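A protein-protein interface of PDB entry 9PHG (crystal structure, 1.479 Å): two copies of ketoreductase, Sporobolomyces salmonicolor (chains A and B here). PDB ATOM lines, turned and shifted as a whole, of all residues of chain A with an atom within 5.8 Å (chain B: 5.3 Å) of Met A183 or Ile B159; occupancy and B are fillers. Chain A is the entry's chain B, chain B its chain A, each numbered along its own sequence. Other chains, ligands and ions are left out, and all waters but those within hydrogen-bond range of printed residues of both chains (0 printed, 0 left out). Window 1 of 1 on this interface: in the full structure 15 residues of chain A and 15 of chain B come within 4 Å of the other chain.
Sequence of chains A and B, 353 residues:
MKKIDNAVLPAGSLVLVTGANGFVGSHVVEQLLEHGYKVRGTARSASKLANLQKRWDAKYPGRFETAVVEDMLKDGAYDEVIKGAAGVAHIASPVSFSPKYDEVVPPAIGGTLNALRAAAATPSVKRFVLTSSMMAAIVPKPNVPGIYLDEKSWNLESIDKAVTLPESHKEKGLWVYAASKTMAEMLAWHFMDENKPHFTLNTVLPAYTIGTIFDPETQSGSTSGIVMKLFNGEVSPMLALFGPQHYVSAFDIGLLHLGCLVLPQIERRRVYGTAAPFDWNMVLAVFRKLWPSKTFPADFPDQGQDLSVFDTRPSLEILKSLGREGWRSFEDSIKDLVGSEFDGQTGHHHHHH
The side-chain hydroxyl of Thr B164 lies within hydrogen-bond range of the side-chain carboxylate of Asp B160, 2.7 Å away.
Printed residues of chain B that touch a printed residue of chain A: Leu B156, Ile B159, Asp B160, Val B163, Thr B164 and Met B183. Hydrophobic or aromatic side chains of chain B that line the printed part of chain A: Leu B156, Ile B159, Val B163 and Met B183. Printed residues of chain A that touch a printed residue of chain B: Ile A109, Ile A159, Met A183 and Leu A187. Along chain A the printed residues that touch a printed residue of chain B span positions 109 to 187.
Among the printed residues, pairs that only touch across the chains: Ile A109 with Val B163, Ile A109 with Thr B164, Ile A159 with Met B183, Met A183 with Ile B159, Leu A187 with Leu B156 and Leu A187 with Asp B160.
Of the printed residues of chain B, Ile A109 touches Val B163 and Thr B164. Met A186 touches none of the printed residues of chain B. Printed residues of chain A within 4 Å of Ile B159: Met A183 (3.8 Å). Of the printed residues of chain A, Asp B160 touches Leu A187 (3.8 Å). Of the printed residues of chain A, Val B163 touches Ile A109 (3.8 Å). The nearest printed residue of chain A that does not touch Ile B159 is Leu A187 (4.1 Å).
Ile A159 touches Met B183, and with the chains exchanged Met A183 touches Ile B159. Positions printed for both chains: 159, 179, 182, 183 and 186. Of the 6 pairs that touch across the chains among the printed residues, 2 have their exchanged pair printed and touching as well.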
ATOM      1  N   TYR A 101      32.538 -20.310  24.867  1.00  0.00           N
ATOM      2  CA  TYR A 101      32.109 -18.909  24.796  1.00  0.00           C
ATOM      3  C   TYR A 101      31.622 -18.514  23.370  1.00  0.00           C
ATOM      4  O   TYR A 101      30.538 -17.916  23.214  1.00  0.00           O
ATOM      5  CB  TYR A 101      33.296 -18.025  25.224  1.00  0.00           C
ATOM      6  CG  TYR A 101      32.959 -16.567  25.387  1.00  0.00           C
ATOM      7  CD1 TYR A 101      32.977 -15.709  24.299  1.00  0.00           C
ATOM      8  CD2 TYR A 101      32.799 -16.009  26.651  1.00  0.00           C
ATOM      9  CE1 TYR A 101      32.751 -14.351  24.449  1.00  0.00           C
ATOM     10  CE2 TYR A 101      32.586 -14.651  26.815  1.00  0.00           C
ATOM     11  CZ  TYR A 101      32.596 -13.816  25.714  1.00  0.00           C
ATOM     12  OH  TYR A 101      32.501 -12.456  25.894  1.00  0.00           O
ATOM     13  N   VAL A 105      27.795 -16.759  23.298  1.00  0.00           N
ATOM     14  CA  VAL A 105      27.700 -15.306  23.342  1.00  0.00           C
ATOM     15  C   VAL A 105      27.370 -14.693  21.965  1.00  0.00           C
ATOM     16  O   VAL A 105      26.435 -13.853  21.894  1.00  0.00           O
ATOM     17  CB  VAL A 105      28.989 -14.730  24.001  1.00  0.00           C
ATOM     18  CG1 VAL A 105      29.028 -13.225  23.869  1.00  0.00           C
ATOM     19  CG2 VAL A 105      29.067 -15.143  25.478  1.00  0.00           C
ATOM     20  N   ILE A 109      23.917 -12.305  21.344  1.00  0.00           N
ATOM     21  CA  ILE A 109      23.971 -10.892  20.995  1.00  0.00           C
ATOM     22  C   ILE A 109      23.436 -10.665  19.582  1.00  0.00           C
ATOM     23  O   ILE A 109      22.638  -9.730  19.369  1.00  0.00           O
ATOM     24  CB  ILE A 109      25.422 -10.339  21.210  1.00  0.00           C
ATOM     25  CG1 ILE A 109      25.696 -10.240  22.729  1.00  0.00           C
ATOM     26  CG2 ILE A 109      25.566  -8.957  20.494  1.00  0.00           C
ATOM     27  CD1 ILE A 109      27.183 -10.108  23.129  1.00  0.00           C
ATOM     28  N   ILE A 159      30.688 -11.037  33.196  1.00  0.00           N
ATOM     29  CA  ILE A 159      31.517 -10.678  32.040  1.00  0.00           C
ATOM     30  C   ILE A 159      32.959 -11.117  32.330  1.00  0.00           C
ATOM     31  O   ILE A 159      33.570 -11.808  31.506  1.00  0.00           O
ATOM     32  CB  ILE A 159      31.355  -9.199  31.670  1.00  0.00           C
ATOM     33  CG1 ILE A 159      29.865  -8.932  31.279  1.00  0.00           C
ATOM     34  CG2 ILE A 159      32.292  -8.865  30.485  1.00  0.00           C
ATOM     35  CD1 ILE A 159      29.548  -7.497  30.894  1.00  0.00           C
ATOM     36  N   ALA A 178      25.383 -16.654  31.765  1.00  0.00           N
ATOM     37  CA  ALA A 178      25.019 -15.397  32.422  1.00  0.00           C
ATOM     38  C   ALA A 178      25.570 -14.166  31.654  1.00  0.00           C
ATOM     39  O   ALA A 178      24.861 -13.159  31.463  1.00  0.00           O
ATOM     40  CB  ALA A 178      25.528 -15.388  33.848  1.00  0.00           C
ATOM     41  N   ALA A 179      26.826 -14.250  31.197  1.00  0.00           N
ATOM     42  CA  ALA A 179      27.419 -13.127  30.437  1.00  0.00           C
ATOM     43  C   ALA A 179      26.681 -12.904  29.128  1.00  0.00           C
ATOM     44  O   ALA A 179      26.517 -11.765  28.715  1.00  0.00           O
ATOM     45  CB  ALA A 179      28.883 -13.405  30.176  1.00  0.00           C
ATOM     46  N   SER A 180      26.267 -13.968  28.441  1.00  0.00           N
ATOM     47  CA  SER A 180      25.543 -13.824  27.168  1.00  0.00           C
ATOM     48  C   SER A 180      24.233 -13.064  27.405  1.00  0.00           C
ATOM     49  O   SER A 180      23.872 -12.185  26.600  1.00  0.00           O
ATOM     50  CB  SER A 180      25.300 -15.201  26.539  1.00  0.00           C
ATOM     51  OG  SER A 180      24.237 -15.935  27.141  1.00  0.00           O
ATOM     52  N   LYS A 181      23.542 -13.347  28.519  1.00  0.00           N
ATOM     53  CA  LYS A 181      22.273 -12.658  28.803  1.00  0.00           C
ATOM     54  C   LYS A 181      22.536 -11.221  29.190  1.00  0.00           C
ATOM     55  O   LYS A 181      21.825 -10.309  28.768  1.00  0.00           O
ATOM     56  CB  LYS A 181      21.535 -13.378  29.964  1.00  0.00           C
ATOM     57  CG  LYS A 181      21.154 -14.851  29.684  1.00  0.00           C
ATOM     58  CD  LYS A 181      20.368 -15.085  28.386  1.00  0.00           C
ATOM     59  CE  LYS A 181      19.051 -14.307  28.386  1.00  0.00           C
ATOM     60  NZ  LYS A 181      18.262 -14.582  27.156  1.00  0.00           N
ATOM     61  N   THR A 182      23.563 -11.012  30.034  1.00  0.00           N
ATOM     62  CA  THR A 182      23.919  -9.670  30.486  1.00  0.00           C
ATOM     63  C   THR A 182      24.288  -8.766  29.307  1.00  0.00           C
ATOM     64  O   THR A 182      23.729  -7.693  29.181  1.00  0.00           O
ATOM     65  CB  THR A 182      25.124  -9.749  31.480  1.00  0.00           C
ATOM     66  OG1 THR A 182      24.759 -10.569  32.594  1.00  0.00           O
ATOM     67  CG2 THR A 182      25.525  -8.367  31.990  1.00  0.00           C
ATOM     68  N   MET A 183      25.172  -9.229  28.414  1.00  0.00           N
ATOM     69  CA  MET A 183      25.615  -8.383  27.320  1.00  0.00           C
ATOM     70  C   MET A 183      24.523  -8.215  26.286  1.00  0.00           C
ATOM     71  O   MET A 183      24.365  -7.113  25.779  1.00  0.00           O
ATOM     72  CB  MET A 183      26.874  -8.961  26.686  1.00  0.00           C
ATOM     73  CG  MET A 183      28.066  -8.767  27.616  1.00  0.00           C
ATOM     74  SD  MET A 183      29.633  -9.242  26.893  1.00  0.00           S
ATOM     75  CE  MET A 183      29.377 -10.877  26.987  1.00  0.00           C
ATOM     76  N   ALA A 184      23.740  -9.281  25.981  1.00  0.00           N
ATOM     77  CA  ALA A 184      22.662  -9.112  24.988  1.00  0.00           C
ATOM     78  C   ALA A 184      21.645  -8.095  25.482  1.00  0.00           C
ATOM     79  O   ALA A 184      21.221  -7.243  24.708  1.00  0.00           O
ATOM     80  CB  ALA A 184      21.956 -10.439  24.703  1.00  0.00           C
ATOM     81  N   GLU A 185      21.276  -8.166  26.804  1.00  0.00           N
ATOM     82  CA  GLU A 185      20.296  -7.190  27.293  1.00  0.00           C
ATOM     83  C   GLU A 185      20.867  -5.776  27.362  1.00  0.00           C
ATOM     84  O   GLU A 185      20.180  -4.818  26.985  1.00  0.00           O
ATOM     85  CB  GLU A 185      19.717  -7.603  28.654  1.00  0.00           C
ATOM     86  CG  GLU A 185      18.436  -6.814  28.924  1.00  0.00           C
ATOM     87  CD  GLU A 185      17.998  -6.790  30.365  1.00  0.00           C
ATOM     88  OE1 GLU A 185      18.491  -7.604  31.181  1.00  0.00           O
ATOM     89  OE2 GLU A 185      17.121  -5.949  30.654  1.00  0.00           O
ATOM     90  N   MET A 186      22.138  -5.631  27.765  1.00  0.00           N
ATOM     91  CA  MET A 186      22.762  -4.306  27.785  1.00  0.00           C
ATOM     92  C   MET A 186      22.738  -3.668  26.369  1.00  0.00           C
ATOM     93  O   MET A 186      22.456  -2.474  26.197  1.00  0.00           O
ATOM     94  CB  MET A 186      24.226  -4.416  28.197  1.00  0.00           C
ATOM     95  CG  MET A 186      24.462  -4.540  29.678  1.00  0.00           C
ATOM     96  SD  MET A 186      26.237  -4.903  29.995  1.00  0.00           S
ATOM     97  CE  MET A 186      26.958  -3.593  29.221  1.00  0.00           C
ATOM     98  N   LEU A 187      23.059  -4.493  25.356  1.00  0.00           N
ATOM     99  CA  LEU A 187      23.115  -4.007  23.986  1.00  0.00           C
ATOM    100  C   LEU A 187      21.736  -3.725  23.427  1.00  0.00           C
ATOM    101  O   LEU A 187      21.610  -2.822  22.607  1.00  0.00           O
ATOM    102  CB  LEU A 187      23.871  -5.018  23.112  1.00  0.00           C
ATOM    103  CG  LEU A 187      25.384  -5.087  23.398  1.00  0.00           C
ATOM    104  CD1 LEU A 187      26.027  -6.156  22.558  1.00  0.00           C
ATOM    105  CD2 LEU A 187      26.053  -3.727  23.144  1.00  0.00           C
ATOM    106  N   ALA A 188      20.686  -4.413  23.920  1.00  0.00           N
ATOM    107  CA  ALA A 188      19.320  -4.088  23.510  1.00  0.00           C
ATOM    108  C   ALA A 188      18.951  -2.680  23.988  1.00  0.00           C
ATOM    109  O   ALA A 188      18.449  -1.871  23.191  1.00  0.00           O
ATOM    110  CB  ALA A 188      18.343  -5.113  24.080  1.00  0.00           C
ATOM    111  N   ASN B 155      32.182   2.262  24.596  1.00  0.00           N
ATOM    112  CA  ASN B 155      32.056   1.711  23.256  1.00  0.00           C
ATOM    113  C   ASN B 155      31.258   0.403  23.278  1.00  0.00           C
ATOM    114  O   ASN B 155      31.785  -0.678  23.006  1.00  0.00           O
ATOM    115  CB  ASN B 155      33.460   1.531  22.640  1.00  0.00           C
ATOM    116  CG  ASN B 155      33.403   1.268  21.152  1.00  0.00           C
ATOM    117  OD1 ASN B 155      32.324   1.044  20.558  1.00  0.00           O
ATOM    118  ND2 ASN B 155      34.563   1.261  20.508  1.00  0.00           N
ATOM    119  N   LEU B 156      29.947   0.539  23.487  1.00  0.00           N
ATOM    120  CA  LEU B 156      29.064  -0.633  23.450  1.00  0.00           C
ATOM    121  C   LEU B 156      28.954  -1.186  22.048  1.00  0.00           C
ATOM    122  O   LEU B 156      28.804  -2.403  21.896  1.00  0.00           O
ATOM    123  CB  LEU B 156      27.687  -0.288  24.042  1.00  0.00           C
ATOM    124  CG  LEU B 156      27.738   0.245  25.501  1.00  0.00           C
ATOM    125  CD1 LEU B 156      26.315   0.476  26.027  1.00  0.00           C
ATOM    126  CD2 LEU B 156      28.516  -0.705  26.461  1.00  0.00           C
ATOM    127  N   GLU B 157      29.159  -0.359  20.990  1.00  0.00           N
ATOM    128  CA  GLU B 157      29.154  -0.875  19.615  1.00  0.00           C
ATOM    129  C   GLU B 157      30.254  -1.974  19.460  1.00  0.00           C
ATOM    130  O   GLU B 157      30.028  -2.984  18.761  1.00  0.00           O
ATOM    131  CB  GLU B 157      29.471   0.276  18.630  1.00  0.00           C
ATOM    132  CG  GLU B 157      29.607  -0.168  17.182  1.00  0.00           C
ATOM    133  CD  GLU B 157      29.733   0.978  16.198  1.00  0.00           C
ATOM    134  OE1 GLU B 157      30.340   2.010  16.561  1.00  0.00           O
ATOM    135  OE2 GLU B 157      29.250   0.827  15.052  1.00  0.00           O
ATOM    136  N   SER B 158      31.407  -1.806  20.116  1.00  0.00           N
ATOM    137  CA  SER B 158      32.478  -2.806  19.978  1.00  0.00           C
ATOM    138  C   SER B 158      32.139  -4.146  20.605  1.00  0.00           C
ATOM    139  O   SER B 158      32.608  -5.186  20.112  1.00  0.00           O
ATOM    140  CB  SER B 158      33.781  -2.281  20.552  1.00  0.00           C
ATOM    141  OG  SER B 158      33.785  -2.213  21.966  1.00  0.00           O
ATOM    142  N   ILE B 159      31.357  -4.145  21.689  1.00  0.00           N
ATOM    143  CA  ILE B 159      30.986  -5.405  22.331  1.00  0.00           C
ATOM    144  C   ILE B 159      30.140  -6.226  21.318  1.00  0.00           C
ATOM    145  O   ILE B 159      30.474  -7.397  21.097  1.00  0.00           O
ATOM    146  CB  ILE B 159      30.330  -5.187  23.716  1.00  0.00           C
ATOM    147  CG1 ILE B 159      31.374  -4.568  24.714  1.00  0.00           C
ATOM    148  CG2 ILE B 159      29.785  -6.543  24.257  1.00  0.00           C
ATOM    149  CD1 ILE B 159      30.808  -4.029  26.044  1.00  0.00           C
ATOM    150  N   ASP B 160      29.227  -5.548  20.547  1.00  0.00           N
ATOM    151  CA  ASP B 160      28.439  -6.196  19.501  1.00  0.00           C
ATOM    152  C   ASP B 160      29.418  -6.697  18.378  1.00  0.00           C
ATOM    153  O   ASP B 160      29.509  -7.894  18.109  1.00  0.00           O
ATOM    154  CB  ASP B 160      27.401  -5.196  18.896  1.00  0.00           C
ATOM    155  CG  ASP B 160      26.873  -5.542  17.513  1.00  0.00           C
ATOM    156  OD1 ASP B 160      26.934  -6.724  17.134  1.00  0.00           O
ATOM    157  OD2 ASP B 160      26.365  -4.630  16.821  1.00  0.00           O
ATOM    158  N   LYS B 161      30.145  -5.783  17.747  1.00  0.00           N
ATOM    159  CA  LYS B 161      30.946  -6.123  16.555  1.00  0.00           C
ATOM    160  C   LYS B 161      32.042  -7.141  16.822  1.00  0.00           C
ATOM    161  O   LYS B 161      32.261  -8.048  16.006  1.00  0.00           O
ATOM    162  CB  LYS B 161      31.511  -4.845  15.920  1.00  0.00           C
ATOM    163  CG  LYS B 161      30.396  -3.966  15.333  1.00  0.00           C
ATOM    164  CD  LYS B 161      30.895  -2.898  14.418  1.00  0.00           C
ATOM    165  CE  LYS B 161      29.771  -2.193  13.692  1.00  0.00           C
ATOM    166  NZ  LYS B 161      30.321  -1.207  12.710  1.00  0.00           N
ATOM    167  N   ALA B 162      32.679  -7.055  17.974  1.00  0.00           N
ATOM    168  CA  ALA B 162      33.746  -8.018  18.305  1.00  0.00           C
ATOM    169  C   ALA B 162      33.252  -9.444  18.334  1.00  0.00           C
ATOM    170  O   ALA B 162      34.017 -10.342  17.997  1.00  0.00           O
ATOM    171  CB  ALA B 162      34.362  -7.676  19.632  1.00  0.00           C
ATOM    172  N   VAL B 163      32.010  -9.664  18.770  1.00  0.00           N
ATOM    173  CA  VAL B 163      31.470 -11.033  18.795  1.00  0.00           C
ATOM    174  C   VAL B 163      30.693 -11.415  17.550  1.00  0.00           C
ATOM    175  O   VAL B 163      30.682 -12.599  17.194  1.00  0.00           O
ATOM    176  CB  VAL B 163      30.630 -11.342  20.049  1.00  0.00           C
ATOM    177  CG1 VAL B 163      31.443 -11.131  21.315  1.00  0.00           C
ATOM    178  CG2 VAL B 163      29.322 -10.568  20.083  1.00  0.00           C
ATOM    179  N   THR B 164      29.963 -10.474  16.925  1.00  0.00           N
ATOM    180  CA  THR B 164      29.076 -10.829  15.802  1.00  0.00           C
ATOM    181  C   THR B 164      29.728 -10.794  14.432  1.00  0.00           C
ATOM    182  O   THR B 164      29.222 -11.479  13.529  1.00  0.00           O
ATOM    183  CB  THR B 164      27.824  -9.934  15.799  1.00  0.00           C
ATOM    184  OG1 THR B 164      28.230  -8.582  15.585  1.00  0.00           O
ATOM    185  CG2 THR B 164      27.042 -10.042  17.104  1.00  0.00           C
ATOM    186  N   ALA B 179      36.794  -3.945  21.818  1.00  0.00           N
ATOM    187  CA  ALA B 179      35.982  -4.595  22.859  1.00  0.00           C
ATOM    188  C   ALA B 179      36.847  -4.984  24.059  1.00  0.00           C
ATOM    189  O   ALA B 179      36.426  -4.826  25.197  1.00  0.00           O
ATOM    190  CB  ALA B 179      35.281  -5.824  22.295  1.00  0.00           C
ATOM    191  N   THR B 182      37.375  -1.827  26.063  1.00  0.00           N
ATOM    192  CA  THR B 182      36.107  -1.426  26.631  1.00  0.00           C
ATOM    193  C   THR B 182      35.731  -2.298  27.839  1.00  0.00           C
ATOM    194  O   THR B 182      35.457  -1.764  28.918  1.00  0.00           O
ATOM    195  CB  THR B 182      34.990  -1.520  25.577  1.00  0.00           C
ATOM    196  OG1 THR B 182      35.325  -0.678  24.475  1.00  0.00           O
ATOM    197  CG2 THR B 182      33.642  -1.102  26.143  1.00  0.00           C
ATOM    198  N   MET B 183      35.813  -3.632  27.687  1.00  0.00           N
ATOM    199  CA  MET B 183      35.403  -4.558  28.750  1.00  0.00           C
ATOM    200  C   MET B 183      36.399  -4.532  29.910  1.00  0.00           C
ATOM    201  O   MET B 183      35.995  -4.485  31.090  1.00  0.00           O
ATOM    202  CB  MET B 183      35.270  -5.976  28.179  1.00  0.00           C
ATOM    203  CG  MET B 183      34.260  -6.067  27.078  1.00  0.00           C
ATOM    204  SD  MET B 183      34.393  -7.624  26.100  1.00  0.00           S
ATOM    205  CE  MET B 183      33.729  -8.728  27.223  1.00  0.00           C
ATOM    206  N   MET B 186      35.773  -1.215  31.771  1.00  0.00           N
ATOM    207  CA  MET B 186      34.499  -1.309  32.518  1.00  0.00           C
ATOM    208  C   MET B 186      34.650  -2.184  33.779  1.00  0.00           C
ATOM    209  O   MET B 186      34.133  -1.838  34.848  1.00  0.00           O
ATOM    210  CB  MET B 186      33.428  -1.983  31.648  1.00  0.00           C
ATOM    211  CG  MET B 186      32.868  -1.101  30.580  1.00  0.00           C
ATOM    212  SD  MET B 186      31.603  -1.986  29.594  1.00  0.00           S
ATOM    213  CE  MET B 186      30.522  -2.360  30.795  1.00  0.00           C
